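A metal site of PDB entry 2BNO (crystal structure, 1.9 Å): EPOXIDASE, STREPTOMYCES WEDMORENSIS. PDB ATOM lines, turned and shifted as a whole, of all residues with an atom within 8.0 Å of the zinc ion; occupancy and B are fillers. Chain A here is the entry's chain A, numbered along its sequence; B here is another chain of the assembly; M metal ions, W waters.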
ATOM      1  N   LEU A 120     -14.651 -21.858  -1.662  1.00  0.00           N
ATOM      2  CA  LEU A 120     -14.922 -22.149  -3.081  1.00  0.00           C
ATOM      3  C   LEU A 120     -13.602 -22.390  -3.790  1.00  0.00           C
ATOM      4  O   LEU A 120     -12.578 -21.834  -3.408  1.00  0.00           O
ATOM      5  CB  LEU A 120     -15.575 -20.941  -3.763  1.00  0.00           C
ATOM      6  CG  LEU A 120     -16.832 -20.354  -3.129  1.00  0.00           C
ATOM      7  CD1 LEU A 120     -17.175 -18.987  -3.745  1.00  0.00           C
ATOM      8  CD2 LEU A 120     -17.991 -21.373  -3.233  1.00  0.00           C
ATOM      9  N   VAL A 122     -12.574 -21.169  -7.320  1.00  0.00           N
ATOM     10  CA  VAL A 122     -13.067 -20.334  -8.385  1.00  0.00           C
ATOM     11  C   VAL A 122     -12.185 -20.529  -9.604  1.00  0.00           C
ATOM     12  O   VAL A 122     -10.958 -20.312  -9.570  1.00  0.00           O
ATOM     13  CB  VAL A 122     -13.115 -18.830  -7.964  1.00  0.00           C
ATOM     14  CG1 VAL A 122     -13.788 -17.979  -9.021  1.00  0.00           C
ATOM     15  CG2 VAL A 122     -13.783 -18.621  -6.593  1.00  0.00           C
ATOM     16  N   ASN A 135     -17.659  -6.478  -7.195  1.00  0.00           N
ATOM     17  CA  ASN A 135     -18.762  -6.644  -6.278  1.00  0.00           C
ATOM     18  C   ASN A 135     -18.833  -5.427  -5.345  1.00  0.00           C
ATOM     19  O   ASN A 135     -18.200  -4.393  -5.605  1.00  0.00           O
ATOM     20  CB  ASN A 135     -18.615  -7.937  -5.513  1.00  0.00           C
ATOM     21  CG  ASN A 135     -17.451  -7.937  -4.599  1.00  0.00           C
ATOM     22  OD1 ASN A 135     -16.905  -6.868  -4.229  1.00  0.00           O
ATOM     23  ND2 ASN A 135     -17.051  -9.122  -4.194  1.00  0.00           N
ATOM     24  N   GLY A 137     -18.417  -5.751  -1.844  1.00  0.00           N
ATOM     25  CA  GLY A 137     -17.874  -6.143  -0.539  1.00  0.00           C
ATOM     26  C   GLY A 137     -18.710  -7.217   0.140  1.00  0.00           C
ATOM     27  O   GLY A 137     -19.932  -7.265  -0.051  1.00  0.00           O
ATOM     28  N   HIS A 138     -18.053  -8.087   0.897  1.00  0.00           N
ATOM     29  CA  HIS A 138     -18.725  -9.101   1.723  1.00  0.00           C
ATOM     30  C   HIS A 138     -19.063  -8.612   3.093  1.00  0.00           C
ATOM     31  O   HIS A 138     -18.538  -7.586   3.553  1.00  0.00           O
ATOM     32  CB  HIS A 138     -17.853 -10.357   1.851  1.00  0.00           C
ATOM     33  CG  HIS A 138     -17.442 -10.899   0.531  1.00  0.00           C
ATOM     34  ND1 HIS A 138     -18.366 -11.319  -0.402  1.00  0.00           N
ATOM     35  CD2 HIS A 138     -16.232 -11.030  -0.048  1.00  0.00           C
ATOM     36  CE1 HIS A 138     -17.738 -11.709  -1.488  1.00  0.00           C
ATOM     37  NE2 HIS A 138     -16.437 -11.540  -1.302  1.00  0.00           N
ATOM     38  N   GLY A 140     -18.463 -10.528   5.655  1.00  0.00           N
ATOM     39  CA  GLY A 140     -17.365 -11.061   6.486  1.00  0.00           C
ATOM     40  C   GLY A 140     -16.015 -10.985   5.748  1.00  0.00           C
ATOM     41  O   GLY A 140     -15.938 -10.521   4.596  1.00  0.00           O
ATOM     42  N   ASN A 141     -14.961 -11.427   6.409  1.00  0.00           N
ATOM     43  CA  ASN A 141     -13.631 -11.397   5.802  1.00  0.00           C
ATOM     44  C   ASN A 141     -13.453 -12.516   4.777  1.00  0.00           C
ATOM     45  O   ASN A 141     -14.252 -13.473   4.734  1.00  0.00           O
ATOM     46  CB  ASN A 141     -12.548 -11.493   6.888  1.00  0.00           C
ATOM     47  CG  ASN A 141     -12.608 -10.318   7.852  1.00  0.00           C
ATOM     48  OD1 ASN A 141     -12.967  -9.213   7.477  1.00  0.00           O
ATOM     49  ND2 ASN A 141     -12.270 -10.568   9.118  1.00  0.00           N
ATOM     50  N   GLU A 142     -12.401 -12.413   3.968  1.00  0.00           N
ATOM     51  CA  GLU A 142     -12.107 -13.449   2.982  1.00  0.00           C
ATOM     52  C   GLU A 142     -10.632 -13.704   2.914  1.00  0.00           C
ATOM     53  O   GLU A 142      -9.861 -12.747   2.925  1.00  0.00           O
ATOM     54  CB  GLU A 142     -12.630 -13.024   1.592  1.00  0.00           C
ATOM     55  CG  GLU A 142     -12.477 -14.107   0.518  1.00  0.00           C
ATOM     56  CD  GLU A 142     -13.182 -13.716  -0.784  1.00  0.00           C
ATOM     57  OE1 GLU A 142     -13.510 -12.522  -0.967  1.00  0.00           O
ATOM     58  OE2 GLU A 142     -13.428 -14.600  -1.619  1.00  0.00           O
ATOM     59  N   PHE A 143     -10.245 -14.992   2.846  1.00  0.00           N
ATOM     60  CA  PHE A 143      -8.868 -15.400   2.618  1.00  0.00           C
ATOM     61  C   PHE A 143      -8.808 -16.022   1.202  1.00  0.00           C
ATOM     62  O   PHE A 143      -9.696 -16.800   0.858  1.00  0.00           O
ATOM     63  CB  PHE A 143      -8.458 -16.467   3.644  1.00  0.00           C
ATOM     64  CG  PHE A 143      -7.214 -17.249   3.229  1.00  0.00           C
ATOM     65  CD1 PHE A 143      -5.937 -16.671   3.354  1.00  0.00           C
ATOM     66  CD2 PHE A 143      -7.323 -18.516   2.656  1.00  0.00           C
ATOM     67  CE1 PHE A 143      -4.799 -17.349   2.919  1.00  0.00           C
ATOM     68  CE2 PHE A 143      -6.188 -19.212   2.229  1.00  0.00           C
ATOM     69  CZ  PHE A 143      -4.925 -18.639   2.361  1.00  0.00           C
ATOM     70  N   LEU A 144      -7.784 -15.665   0.402  1.00  0.00           N
ATOM     71  CA  LEU A 144      -7.652 -16.220  -0.995  1.00  0.00           C
ATOM     72  C   LEU A 144      -6.250 -16.790  -1.206  1.00  0.00           C
ATOM     73  O   LEU A 144      -5.285 -16.295  -0.617  1.00  0.00           O
ATOM     74  CB  LEU A 144      -7.960 -15.142  -2.040  1.00  0.00           C
ATOM     75  CG  LEU A 144      -9.411 -14.622  -2.040  1.00  0.00           C
ATOM     76  CD1 LEU A 144      -9.443 -13.265  -1.318  1.00  0.00           C
ATOM     77  CD2 LEU A 144     -10.063 -14.572  -3.457  1.00  0.00           C
ATOM     78  N   MET A 153      -5.823  -8.788  -9.490  1.00  0.00           N
ATOM     79  CA  MET A 153      -6.783  -8.408  -8.489  1.00  0.00           C
ATOM     80  C   MET A 153      -6.991  -6.876  -8.472  1.00  0.00           C
ATOM     81  O   MET A 153      -6.028  -6.098  -8.618  1.00  0.00           O
ATOM     82  CB  MET A 153      -6.329  -8.913  -7.098  1.00  0.00           C
ATOM     83  CG  MET A 153      -7.205  -8.485  -5.927  1.00  0.00           C
ATOM     84  SD  MET A 153      -8.834  -9.269  -5.947  1.00  0.00           S
ATOM     85  CE  MET A 153      -8.394 -10.989  -5.713  1.00  0.00           C
ATOM     86  N   MET A 172      -3.941 -13.762  -0.057  1.00  0.00           N
ATOM     87  CA  MET A 172      -4.520 -12.451   0.125  1.00  0.00           C
ATOM     88  C   MET A 172      -5.590 -12.490   1.201  1.00  0.00           C
ATOM     89  O   MET A 172      -6.258 -13.516   1.397  1.00  0.00           O
ATOM     90  CB  MET A 172      -5.094 -11.960  -1.190  1.00  0.00           C
ATOM     91  CG  MET A 172      -5.750 -10.638  -1.101  1.00  0.00           C
ATOM     92  SD  MET A 172      -6.051 -10.060  -2.765  1.00  0.00           S
ATOM     93  CE  MET A 172      -7.584  -9.184  -2.558  1.00  0.00           C
ATOM     94  N   VAL A 174      -8.956 -10.097   2.334  1.00  0.00           N
ATOM     95  CA  VAL A 174      -9.835  -8.982   1.981  1.00  0.00           C
ATOM     96  C   VAL A 174     -10.778  -8.755   3.157  1.00  0.00           C
ATOM     97  O   VAL A 174     -11.534  -9.687   3.572  1.00  0.00           O
ATOM     98  CB  VAL A 174     -10.697  -9.297   0.702  1.00  0.00           C
ATOM     99  CG1 VAL A 174     -11.581  -8.098   0.337  1.00  0.00           C
ATOM    100  CG2 VAL A 174      -9.807  -9.621  -0.479  1.00  0.00           C
ATOM    101  N   GLU A 175     -10.737  -7.550   3.722  1.00  0.00           N
ATOM    102  CA  GLU A 175     -11.592  -7.250   4.887  1.00  0.00           C
ATOM    103  C   GLU A 175     -13.056  -7.131   4.489  1.00  0.00           C
ATOM    104  O   GLU A 175     -13.361  -6.773   3.366  1.00  0.00           O
ATOM    105  CB  GLU A 175     -11.140  -5.978   5.607  1.00  0.00           C
ATOM    106  CG  GLU A 175     -11.623  -5.884   7.068  1.00  0.00           C
ATOM    107  CD  GLU A 175     -10.940  -4.729   7.816  1.00  0.00           C
ATOM    108  OE1 GLU A 175     -10.847  -3.621   7.266  1.00  0.00           O
ATOM    109  OE2 GLU A 175     -10.464  -4.978   8.934  1.00  0.00           O
ATOM    110  N   VAL A 178     -15.047  -4.595   1.687  1.00  0.00           N
ATOM    111  CA  VAL A 178     -14.136  -4.021   0.683  1.00  0.00           C
ATOM    112  C   VAL A 178     -14.500  -4.519  -0.704  1.00  0.00           C
ATOM    113  O   VAL A 178     -14.484  -5.725  -0.933  1.00  0.00           O
ATOM    114  CB  VAL A 178     -12.647  -4.378   1.033  1.00  0.00           C
ATOM    115  CG1 VAL A 178     -11.640  -3.960  -0.085  1.00  0.00           C
ATOM    116  CG2 VAL A 178     -12.261  -3.823   2.428  1.00  0.00           C
ATOM    117  N   PRO A 179     -14.836  -3.625  -1.652  1.00  0.00           N
ATOM    118  CA  PRO A 179     -15.165  -4.059  -3.013  1.00  0.00           C
ATOM    119  C   PRO A 179     -13.929  -4.645  -3.673  1.00  0.00           C
ATOM    120  O   PRO A 179     -12.800  -4.174  -3.438  1.00  0.00           O
ATOM    121  CB  PRO A 179     -15.554  -2.742  -3.722  1.00  0.00           C
ATOM    122  CG  PRO A 179     -15.918  -1.811  -2.603  1.00  0.00           C
ATOM    123  CD  PRO A 179     -14.986  -2.166  -1.492  1.00  0.00           C
ATOM    124  N   HIS A 180     -14.116  -5.697  -4.469  1.00  0.00           N
ATOM    125  CA  HIS A 180     -12.996  -6.307  -5.162  1.00  0.00           C
ATOM    126  C   HIS A 180     -13.474  -7.076  -6.377  1.00  0.00           C
ATOM    127  O   HIS A 180     -14.641  -7.449  -6.442  1.00  0.00           O
ATOM    128  CB  HIS A 180     -12.178  -7.223  -4.226  1.00  0.00           C
ATOM    129  CG  HIS A 180     -12.993  -8.268  -3.550  1.00  0.00           C
ATOM    130  ND1 HIS A 180     -13.873  -7.986  -2.523  1.00  0.00           N
ATOM    131  CD2 HIS A 180     -13.067  -9.596  -3.754  1.00  0.00           C
ATOM    132  CE1 HIS A 180     -14.462  -9.099  -2.137  1.00  0.00           C
ATOM    133  NE2 HIS A 180     -14.001 -10.092  -2.873  1.00  0.00           N
ATOM    134  N   ALA A 181     -12.548  -7.268  -7.322  1.00  0.00           N
ATOM    135  CA  ALA A 181     -12.770  -8.018  -8.570  1.00  0.00           C
ATOM    136  C   ALA A 181     -11.477  -8.731  -8.966  1.00  0.00           C
ATOM    137  O   ALA A 181     -10.400  -8.295  -8.587  1.00  0.00           O
ATOM    138  CB  ALA A 181     -13.164  -7.043  -9.665  1.00  0.00           C
ATOM    139  N   PHE A 182     -11.560  -9.827  -9.711  1.00  0.00           N
ATOM    140  CA  PHE A 182     -10.346 -10.397 -10.250  1.00  0.00           C
ATOM    141  C   PHE A 182     -10.588 -10.984 -11.628  1.00  0.00           C
ATOM    142  O   PHE A 182     -11.705 -11.352 -11.992  1.00  0.00           O
ATOM    143  CB  PHE A 182      -9.737 -11.427  -9.303  1.00  0.00           C
ATOM    144  CG  PHE A 182     -10.721 -12.383  -8.718  1.00  0.00           C
ATOM    145  CD1 PHE A 182     -10.975 -13.596  -9.334  1.00  0.00           C
ATOM    146  CD2 PHE A 182     -11.417 -12.069  -7.554  1.00  0.00           C
ATOM    147  CE1 PHE A 182     -11.895 -14.484  -8.799  1.00  0.00           C
ATOM    148  CE2 PHE A 182     -12.325 -12.950  -7.001  1.00  0.00           C
ATOM    149  CZ  PHE A 182     -12.572 -14.159  -7.629  1.00  0.00           C
ATOM    150  N   LEU A 193      -8.388 -19.865  -8.168  1.00  0.00           N
ATOM    151  CA  LEU A 193      -8.017 -19.580  -6.803  1.00  0.00           C
ATOM    152  C   LEU A 193      -8.929 -20.308  -5.842  1.00  0.00           C
ATOM    153  O   LEU A 193     -10.027 -20.811  -6.249  1.00  0.00           O
ATOM    154  CB  LEU A 193      -8.034 -18.076  -6.584  1.00  0.00           C
ATOM    155  CG  LEU A 193      -9.320 -17.376  -6.908  1.00  0.00           C
ATOM    156  CD1 LEU A 193     -10.214 -17.443  -5.706  1.00  0.00           C
ATOM    157  CD2 LEU A 193      -8.994 -15.970  -7.244  1.00  0.00           C
ATOM    158  N   ALA A 195     -11.070 -19.421  -2.612  1.00  0.00           N
ATOM    159  CA  ALA A 195     -11.597 -18.326  -1.845  1.00  0.00           C
ATOM    160  C   ALA A 195     -12.298 -18.879  -0.602  1.00  0.00           C
ATOM    161  O   ALA A 195     -13.232 -19.692  -0.706  1.00  0.00           O
ATOM    162  CB  ALA A 195     -12.573 -17.557  -2.666  1.00  0.00           C
ATOM    163  N   VAL A 196     -11.902 -18.392   0.563  1.00  0.00           N
ATOM    164  CA  VAL A 196     -12.520 -18.836   1.797  1.00  0.00           C
ATOM    165  C   VAL A 196     -13.176 -17.621   2.455  1.00  0.00           C
ATOM    166  O   VAL A 196     -12.513 -16.785   3.069  1.00  0.00           O
ATOM    167  CB  VAL A 196     -11.499 -19.486   2.736  1.00  0.00           C
ATOM    168  CG1 VAL A 196     -12.196 -19.987   4.043  1.00  0.00           C
ATOM    169  CG2 VAL A 196     -10.663 -20.617   2.000  1.00  0.00           C
ATOM    170  N   ASN A 197     -14.489 -17.514   2.329  1.00  0.00           N
ATOM    171  CA  ASN A 197     -15.214 -16.492   3.078  1.00  0.00           C
ATOM    172  C   ASN A 197     -15.484 -17.075   4.465  1.00  0.00           C
ATOM    173  O   ASN A 197     -15.766 -18.256   4.583  1.00  0.00           O
ATOM    174  CB  ASN A 197     -16.504 -16.103   2.338  1.00  0.00           C
ATOM    175  CG  ASN A 197     -16.237 -15.125   1.212  1.00  0.00           C
ATOM    176  OD1 ASN A 197     -16.050 -15.509   0.069  1.00  0.00           O
ATOM    177  ND2 ASN A 197     -16.179 -13.848   1.539  1.00  0.00           N
ATOM    178  N   LYS B  23     -23.843 -19.627  -3.545  1.00  0.00           N
ATOM    179  CA  LYS B  23     -23.772 -19.794  -4.989  1.00  0.00           C
ATOM    180  C   LYS B  23     -24.882 -20.691  -5.547  1.00  0.00           C
ATOM    181  O   LYS B  23     -24.643 -21.510  -6.467  1.00  0.00           O
ATOM    182  CB  LYS B  23     -22.374 -20.292  -5.400  1.00  0.00           C
ATOM    183  CG  LYS B  23     -21.218 -19.429  -4.832  1.00  0.00           C
ATOM    184  CD  LYS B  23     -21.178 -18.097  -5.488  1.00  0.00           C
ATOM    185  CE  LYS B  23     -20.210 -17.135  -4.833  1.00  0.00           C
ATOM    186  NZ  LYS B  23     -20.214 -15.853  -5.606  1.00  0.00           N
HETATM  187 ZN    ZN M   1     -14.711 -12.016  -2.462  1.00  0.00          ZN
HETATM  188  O   HOH W   1     -13.871 -12.988  -3.912  1.00  0.00           O
HETATM  189  O   HOH W   2     -15.945 -14.732  -2.445  1.00  0.00           O
HETATM  190  O   HOH W   3     -16.577 -11.897  -3.987  1.00  0.00           O
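The side-chain carboxylate (OE2) of Glu 142 lies close to the side-chain amide oxygen (OD1) of Asn 197, 3.2 Å away.
N of Val 174 lies within hydrogen-bond range of O of Glu 142, 2.9 Å away.
The backbone NH (N) of His 180 lies within hydrogen-bond range of the side-chain amide oxygen (OD1) of Asn 135 (3.0 Å).
ND1 of His 180 is in hydrogen-bond range of O of Val 178 (2.8 Å).
Of the 24 residues printed, 3 come within 4 Å of the zinc ion.
Water W1 binds the zinc ion (1.9 Å).
OE1 of Glu 142 binds the zinc ion (2.0 Å).
The zinc ion is bound by a ring nitrogen (NE2) of His 180, 2.1 Å away.
NE2 of His 138 is bound to the zinc ion (2.1 Å).
The zinc ion is bound by water W3.
The zinc ion has five donor atoms within binding distance.
Water W2 bridges the side-chain amide oxygen of Asn 197 (2.6 Å) and the side-chain carboxylate of Glu 142 (2.7 Å).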
